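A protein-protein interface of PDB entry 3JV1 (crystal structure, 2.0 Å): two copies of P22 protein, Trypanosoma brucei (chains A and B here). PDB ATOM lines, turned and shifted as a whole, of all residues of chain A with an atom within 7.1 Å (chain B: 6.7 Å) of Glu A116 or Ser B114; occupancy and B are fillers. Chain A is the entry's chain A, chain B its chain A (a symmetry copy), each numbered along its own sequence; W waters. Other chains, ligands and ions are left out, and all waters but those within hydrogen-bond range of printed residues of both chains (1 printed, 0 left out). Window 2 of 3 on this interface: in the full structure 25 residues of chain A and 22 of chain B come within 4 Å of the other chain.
Of the 12 printed residues of chain A, 3 touch a printed residue of chain B.
Hydrophobic or aromatic side chains of chain A within 4 Å of the printed part of chain B: Phe A119.
Hydrophobic or aromatic side chains of chain B that line the printed part of chain A: Ala B115.
Among the printed residues, 5 pairs touch across the chains.
N of Ala B115 lies within hydrogen-bond range of OE2 of Glu A116 (2.6 Å).
Among the printed residues, pairs that only touch across the chains: Ala A115 with Ala B115 (3.6 Å), Glu A116 with Ser B114 (3.5 Å), Phe A119 with Thr B113 (2.8 Å) and Phe A119 with Gln B118 (3.0 Å).
Water W1 lies within hydrogen-bond range of the side-chain carboxylate (OE2) of Glu A116, the backbone NH (N) of Glu B116 and the backbone NH (N) of Ala B115.
Ala A115 touches its own counterpart, Ala B115.
Glu A116 touches Ser B114, but with the chains exchanged Ser A114 does not touch Glu B116 (9.0 Å).
Glu A116 touches Ala B115, but with the chains exchanged Ala A115 does not touch Glu B116 (6.2 Å).
Phe A119 touches Thr B113, but with the chains exchanged Thr A113 does not touch Phe B119 (13.8 Å).
9 positions are printed for both chains.
Of the 5 pairs that touch across the chains among the printed residues, 1 has its exchanged pair printed and touching as well.
The side-chain carboxylate (OE1) of Glu A116 is in hydrogen-bond range of the side-chain amide nitrogen (NE2) of Gln A120 (2.9 Å).
OG of Ser A122 sits at hydrogen-bond distance from O of Phe A119 (2.7 Å).
The side-chain carboxylate (OD1) of Asp B112 is in hydrogen-bond range of the backbone NH (N) of Ser B114 (2.9 Å).
O of Thr B113 lies within hydrogen-bond range of NE2 of Gln B118, 2.6 Å away.
N of Ala B117 lies within hydrogen-bond range of OG of Ser B114.
OE1 of Gln B118 lies close to O of Ser B114 (2.7 Å).
Thr A113 touches none of the printed residues of chain B.
Of the printed residues of chain B, Ala A115 touches Ala B115 (3.6 Å).
Of the printed residues of chain B, Phe A119 touches Thr B113 and Gln B118.
Of the printed residues of chain A, Thr B113 touches Phe A119.
Ser B114 touches just one residue of chain A: Glu A116.
Printed residues of chain A within 4 Å of Ala B115: Ala A115 (3.6 Å) and Glu A116 (2.6 Å).
Printed residues of chain A within 4 Å of Gln B118: Phe A119.
The nearest residue of chain A that does not touch Ser B114 is Phe A119 (4.6 Å).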
ATOM      1  N   LEU A 109     -12.746  -5.050  23.085  1.00  0.00           N
ATOM      2  CA  LEU A 109     -14.151  -5.314  22.825  1.00  0.00           C
ATOM      3  C   LEU A 109     -14.347  -5.465  21.321  1.00  0.00           C
ATOM      4  O   LEU A 109     -15.100  -6.319  20.865  1.00  0.00           O
ATOM      5  CB  LEU A 109     -15.018  -4.172  23.351  1.00  0.00           C
ATOM      6  CG  LEU A 109     -16.519  -4.264  23.063  1.00  0.00           C
ATOM      7  CD1 LEU A 109     -17.109  -5.537  23.653  1.00  0.00           C
ATOM      8  CD2 LEU A 109     -17.200  -3.037  23.654  1.00  0.00           C
ATOM      9  N   ASP A 112     -13.398  -8.910  20.374  1.00  0.00           N
ATOM     10  CA  ASP A 112     -14.252  -9.925  20.968  1.00  0.00           C
ATOM     11  C   ASP A 112     -15.394 -10.253  20.016  1.00  0.00           C
ATOM     12  O   ASP A 112     -16.147  -9.369  19.612  1.00  0.00           O
ATOM     13  CB  ASP A 112     -14.816  -9.411  22.289  1.00  0.00           C
ATOM     14  CG  ASP A 112     -15.407 -10.514  23.141  1.00  0.00           C
ATOM     15  OD1 ASP A 112     -15.891 -11.515  22.573  1.00  0.00           O
ATOM     16  OD2 ASP A 112     -15.396 -10.365  24.382  1.00  0.00           O
ATOM     17  N   THR A 113     -15.530 -11.524  19.658  1.00  0.00           N
ATOM     18  CA  THR A 113     -16.595 -11.922  18.750  1.00  0.00           C
ATOM     19  C   THR A 113     -17.732 -12.696  19.427  1.00  0.00           C
ATOM     20  O   THR A 113     -18.569 -13.272  18.747  1.00  0.00           O
ATOM     21  CB  THR A 113     -16.042 -12.778  17.590  1.00  0.00           C
ATOM     22  OG1 THR A 113     -15.302 -13.882  18.121  1.00  0.00           O
ATOM     23  CG2 THR A 113     -15.132 -11.943  16.698  1.00  0.00           C
ATOM     24  N   SER A 114     -17.773 -12.712  20.757  1.00  0.00           N
ATOM     25  CA  SER A 114     -18.842 -13.428  21.457  1.00  0.00           C
ATOM     26  C   SER A 114     -20.201 -12.773  21.188  1.00  0.00           C
ATOM     27  O   SER A 114     -20.264 -11.634  20.747  1.00  0.00           O
ATOM     28  CB  SER A 114     -18.565 -13.450  22.959  1.00  0.00           C
ATOM     29  OG  SER A 114     -18.637 -12.152  23.517  1.00  0.00           O
ATOM     30  N   ALA A 115     -21.286 -13.493  21.447  1.00  0.00           N
ATOM     31  CA  ALA A 115     -22.618 -12.938  21.222  1.00  0.00           C
ATOM     32  C   ALA A 115     -22.805 -11.729  22.124  1.00  0.00           C
ATOM     33  O   ALA A 115     -23.395 -10.729  21.716  1.00  0.00           O
ATOM     34  CB  ALA A 115     -23.686 -13.979  21.508  1.00  0.00           C
ATOM     35  N   GLU A 116     -22.283 -11.820  23.345  1.00  0.00           N
ATOM     36  CA  GLU A 116     -22.381 -10.722  24.303  1.00  0.00           C
ATOM     37  C   GLU A 116     -21.612  -9.493  23.808  1.00  0.00           C
ATOM     38  O   GLU A 116     -22.093  -8.367  23.930  1.00  0.00           O
ATOM     39  CB  GLU A 116     -21.850 -11.150  25.672  1.00  0.00           C
ATOM     40  CG  GLU A 116     -21.911 -10.038  26.708  1.00  0.00           C
ATOM     41  CD  GLU A 116     -23.303  -9.419  26.821  1.00  0.00           C
ATOM     42  OE1 GLU A 116     -23.399  -8.252  27.253  1.00  0.00           O
ATOM     43  OE2 GLU A 116     -24.298 -10.104  26.486  1.00  0.00           O
ATOM     44  N   ALA A 117     -20.423  -9.707  23.251  1.00  0.00           N
ATOM     45  CA  ALA A 117     -19.627  -8.598  22.733  1.00  0.00           C
ATOM     46  C   ALA A 117     -20.361  -7.929  21.577  1.00  0.00           C
ATOM     47  O   ALA A 117     -20.349  -6.709  21.455  1.00  0.00           O
ATOM     48  CB  ALA A 117     -18.262  -9.090  22.267  1.00  0.00           C
ATOM     49  N   GLN A 118     -20.996  -8.726  20.721  1.00  0.00           N
ATOM     50  CA  GLN A 118     -21.740  -8.171  19.599  1.00  0.00           C
ATOM     51  C   GLN A 118     -22.861  -7.264  20.077  1.00  0.00           C
ATOM     52  O   GLN A 118     -23.083  -6.195  19.514  1.00  0.00           O
ATOM     53  CB  GLN A 118     -22.370  -9.265  18.744  1.00  0.00           C
ATOM     54  CG  GLN A 118     -21.520  -9.763  17.602  1.00  0.00           C
ATOM     55  CD  GLN A 118     -20.441 -10.695  18.063  1.00  0.00           C
ATOM     56  OE1 GLN A 118     -19.389 -10.262  18.535  1.00  0.00           O
ATOM     57  NE2 GLN A 118     -20.698 -11.993  17.947  1.00  0.00           N
ATOM     58  N   PHE A 119     -23.587  -7.696  21.101  1.00  0.00           N
ATOM     59  CA  PHE A 119     -24.681  -6.887  21.596  1.00  0.00           C
ATOM     60  C   PHE A 119     -24.202  -5.550  22.154  1.00  0.00           C
ATOM     61  O   PHE A 119     -24.811  -4.511  21.907  1.00  0.00           O
ATOM     62  CB  PHE A 119     -25.466  -7.626  22.672  1.00  0.00           C
ATOM     63  CG  PHE A 119     -26.551  -6.799  23.270  1.00  0.00           C
ATOM     64  CD1 PHE A 119     -27.676  -6.471  22.522  1.00  0.00           C
ATOM     65  CD2 PHE A 119     -26.419  -6.283  24.553  1.00  0.00           C
ATOM     66  CE1 PHE A 119     -28.658  -5.634  23.039  1.00  0.00           C
ATOM     67  CE2 PHE A 119     -27.393  -5.443  25.083  1.00  0.00           C
ATOM     68  CZ  PHE A 119     -28.519  -5.117  24.321  1.00  0.00           C
ATOM     69  N   GLN A 120     -23.110  -5.575  22.910  1.00  0.00           N
ATOM     70  CA  GLN A 120     -22.576  -4.351  23.489  1.00  0.00           C
ATOM     71  C   GLN A 120     -22.156  -3.365  22.405  1.00  0.00           C
ATOM     72  O   GLN A 120     -22.419  -2.169  22.502  1.00  0.00           O
ATOM     73  CB  GLN A 120     -21.398  -4.677  24.403  1.00  0.00           C
ATOM     74  CG  GLN A 120     -21.819  -5.293  25.732  1.00  0.00           C
ATOM     75  CD  GLN A 120     -20.642  -5.789  26.538  1.00  0.00           C
ATOM     76  OE1 GLN A 120     -19.562  -5.198  26.502  1.00  0.00           O
ATOM     77  NE2 GLN A 120     -20.845  -6.872  27.287  1.00  0.00           N
ATOM     78  N   LYS A 121     -21.507  -3.868  21.366  1.00  0.00           N
ATOM     79  CA  LYS A 121     -21.077  -3.009  20.273  1.00  0.00           C
ATOM     80  C   LYS A 121     -22.252  -2.496  19.434  1.00  0.00           C
ATOM     81  O   LYS A 121     -22.139  -1.459  18.784  1.00  0.00           O
ATOM     82  CB  LYS A 121     -20.062  -3.751  19.394  1.00  0.00           C
ATOM     83  CG  LYS A 121     -18.726  -3.954  20.110  1.00  0.00           C
ATOM     84  CD  LYS A 121     -17.716  -4.746  19.296  1.00  0.00           C
ATOM     85  CE  LYS A 121     -18.021  -6.243  19.289  1.00  0.00           C
ATOM     86  NZ  LYS A 121     -16.884  -7.003  18.702  1.00  0.00           N
ATOM     87  N   SER A 122     -23.378  -3.202  19.459  1.00  0.00           N
ATOM     88  CA  SER A 122     -24.543  -2.779  18.682  1.00  0.00           C
ATOM     89  C   SER A 122     -25.169  -1.502  19.253  1.00  0.00           C
ATOM     90  O   SER A 122     -25.979  -0.849  18.598  1.00  0.00           O
ATOM     91  CB  SER A 122     -25.603  -3.889  18.646  1.00  0.00           C
ATOM     92  OG  SER A 122     -26.367  -3.903  19.841  1.00  0.00           O
ATOM     93  N   LEU B 111     -35.085  -6.838  33.263  1.00  0.00           N
ATOM     94  CA  LEU B 111     -34.063  -5.800  33.391  1.00  0.00           C
ATOM     95  C   LEU B 111     -32.715  -6.207  32.794  1.00  0.00           C
ATOM     96  O   LEU B 111     -31.931  -5.358  32.372  1.00  0.00           O
ATOM     97  CB  LEU B 111     -33.865  -5.446  34.867  1.00  0.00           C
ATOM     98  CG  LEU B 111     -35.012  -4.715  35.555  1.00  0.00           C
ATOM     99  CD1 LEU B 111     -34.716  -4.587  37.033  1.00  0.00           C
ATOM    100  CD2 LEU B 111     -35.193  -3.349  34.930  1.00  0.00           C
ATOM    101  N   ASP B 112     -32.448  -7.505  32.774  1.00  0.00           N
ATOM    102  CA  ASP B 112     -31.195  -8.021  32.244  1.00  0.00           C
ATOM    103  C   ASP B 112     -31.082  -7.670  30.767  1.00  0.00           C
ATOM    104  O   ASP B 112     -31.954  -8.015  29.973  1.00  0.00           O
ATOM    105  CB  ASP B 112     -31.150  -9.536  32.418  1.00  0.00           C
ATOM    106  CG  ASP B 112     -29.758 -10.103  32.238  1.00  0.00           C
ATOM    107  OD1 ASP B 112     -28.965  -9.512  31.476  1.00  0.00           O
ATOM    108  OD2 ASP B 112     -29.469 -11.152  32.852  1.00  0.00           O
ATOM    109  N   THR B 113     -30.007  -6.988  30.393  1.00  0.00           N
ATOM    110  CA  THR B 113     -29.822  -6.611  29.000  1.00  0.00           C
ATOM    111  C   THR B 113     -28.731  -7.413  28.280  1.00  0.00           C
ATOM    112  O   THR B 113     -28.330  -7.050  27.183  1.00  0.00           O
ATOM    113  CB  THR B 113     -29.492  -5.108  28.872  1.00  0.00           C
ATOM    114  OG1 THR B 113     -28.370  -4.793  29.702  1.00  0.00           O
ATOM    115  CG2 THR B 113     -30.687  -4.263  29.295  1.00  0.00           C
ATOM    116  N   SER B 114     -28.253  -8.499  28.880  1.00  0.00           N
ATOM    117  CA  SER B 114     -27.216  -9.307  28.234  1.00  0.00           C
ATOM    118  C   SER B 114     -27.756  -9.962  26.959  1.00  0.00           C
ATOM    119  O   SER B 114     -28.961 -10.047  26.766  1.00  0.00           O
ATOM    120  CB  SER B 114     -26.710 -10.382  29.195  1.00  0.00           C
ATOM    121  OG  SER B 114     -27.716 -11.332  29.485  1.00  0.00           O
ATOM    122  N   ALA B 115     -26.866 -10.422  26.086  1.00  0.00           N
ATOM    123  CA  ALA B 115     -27.301 -11.064  24.849  1.00  0.00           C
ATOM    124  C   ALA B 115     -28.093 -12.315  25.197  1.00  0.00           C
ATOM    125  O   ALA B 115     -29.094 -12.623  24.550  1.00  0.00           O
ATOM    126  CB  ALA B 115     -26.105 -11.422  23.983  1.00  0.00           C
ATOM    127  N   GLU B 116     -27.648 -13.022  26.232  1.00  0.00           N
ATOM    128  CA  GLU B 116     -28.328 -14.236  26.678  1.00  0.00           C
ATOM    129  C   GLU B 116     -29.734 -13.918  27.194  1.00  0.00           C
ATOM    130  O   GLU B 116     -30.683 -14.647  26.906  1.00  0.00           O
ATOM    131  CB  GLU B 116     -27.520 -14.938  27.771  1.00  0.00           C
ATOM    132  CG  GLU B 116     -28.189 -16.202  28.288  1.00  0.00           C
ATOM    133  CD  GLU B 116     -28.560 -17.168  27.165  1.00  0.00           C
ATOM    134  OE1 GLU B 116     -29.485 -17.982  27.364  1.00  0.00           O
ATOM    135  OE2 GLU B 116     -27.919 -17.118  26.088  1.00  0.00           O
ATOM    136  N   ALA B 117     -29.870 -12.834  27.954  1.00  0.00           N
ATOM    137  CA  ALA B 117     -31.177 -12.443  28.474  1.00  0.00           C
ATOM    138  C   ALA B 117     -32.112 -12.095  27.321  1.00  0.00           C
ATOM    139  O   ALA B 117     -33.290 -12.430  27.353  1.00  0.00           O
ATOM    140  CB  ALA B 117     -31.043 -11.250  29.413  1.00  0.00           C
ATOM    141  N   GLN B 118     -31.589 -11.415  26.304  1.00  0.00           N
ATOM    142  CA  GLN B 118     -32.404 -11.060  25.150  1.00  0.00           C
ATOM    143  C   GLN B 118     -32.949 -12.296  24.458  1.00  0.00           C
ATOM    144  O   GLN B 118     -34.111 -12.331  24.063  1.00  0.00           O
ATOM    145  CB  GLN B 118     -31.606 -10.271  24.117  1.00  0.00           C
ATOM    146  CG  GLN B 118     -31.638  -8.772  24.282  1.00  0.00           C
ATOM    147  CD  GLN B 118     -30.741  -8.303  25.385  1.00  0.00           C
ATOM    148  OE1 GLN B 118     -31.107  -8.346  26.561  1.00  0.00           O
ATOM    149  NE2 GLN B 118     -29.543  -7.862  25.020  1.00  0.00           N
ATOM    150  N   PHE B 119     -32.106 -13.308  24.286  1.00  0.00           N
ATOM    151  CA  PHE B 119     -32.557 -14.511  23.618  1.00  0.00           C
ATOM    152  C   PHE B 119     -33.666 -15.217  24.393  1.00  0.00           C
ATOM    153  O   PHE B 119     -34.645 -15.678  23.809  1.00  0.00           O
ATOM    154  CB  PHE B 119     -31.403 -15.481  23.400  1.00  0.00           C
ATOM    155  CG  PHE B 119     -31.836 -16.769  22.791  1.00  0.00           C
ATOM    156  CD1 PHE B 119     -32.265 -16.811  21.468  1.00  0.00           C
ATOM    157  CD2 PHE B 119     -31.889 -17.928  23.555  1.00  0.00           C
ATOM    158  CE1 PHE B 119     -32.748 -17.991  20.912  1.00  0.00           C
ATOM    159  CE2 PHE B 119     -32.371 -19.115  23.011  1.00  0.00           C
ATOM    160  CZ  PHE B 119     -32.803 -19.145  21.682  1.00  0.00           C
ATOM    161  N   LYS B 121     -35.826 -13.923  26.484  1.00  0.00           N
ATOM    162  CA  LYS B 121     -37.055 -13.149  26.391  1.00  0.00           C
ATOM    163  C   LYS B 121     -37.682 -13.208  24.995  1.00  0.00           C
ATOM    164  O   LYS B 121     -38.885 -13.003  24.849  1.00  0.00           O
ATOM    165  CB  LYS B 121     -36.790 -11.697  26.810  1.00  0.00           C
ATOM    166  CG  LYS B 121     -36.513 -11.575  28.309  1.00  0.00           C
ATOM    167  CD  LYS B 121     -36.178 -10.159  28.751  1.00  0.00           C
ATOM    168  CE  LYS B 121     -34.751  -9.758  28.382  1.00  0.00           C
ATOM    169  NZ  LYS B 121     -34.382  -8.478  29.046  1.00  0.00           N
HETATM  170  O   HOH W   1     -24.829 -12.582  27.089  1.00  0.00           O
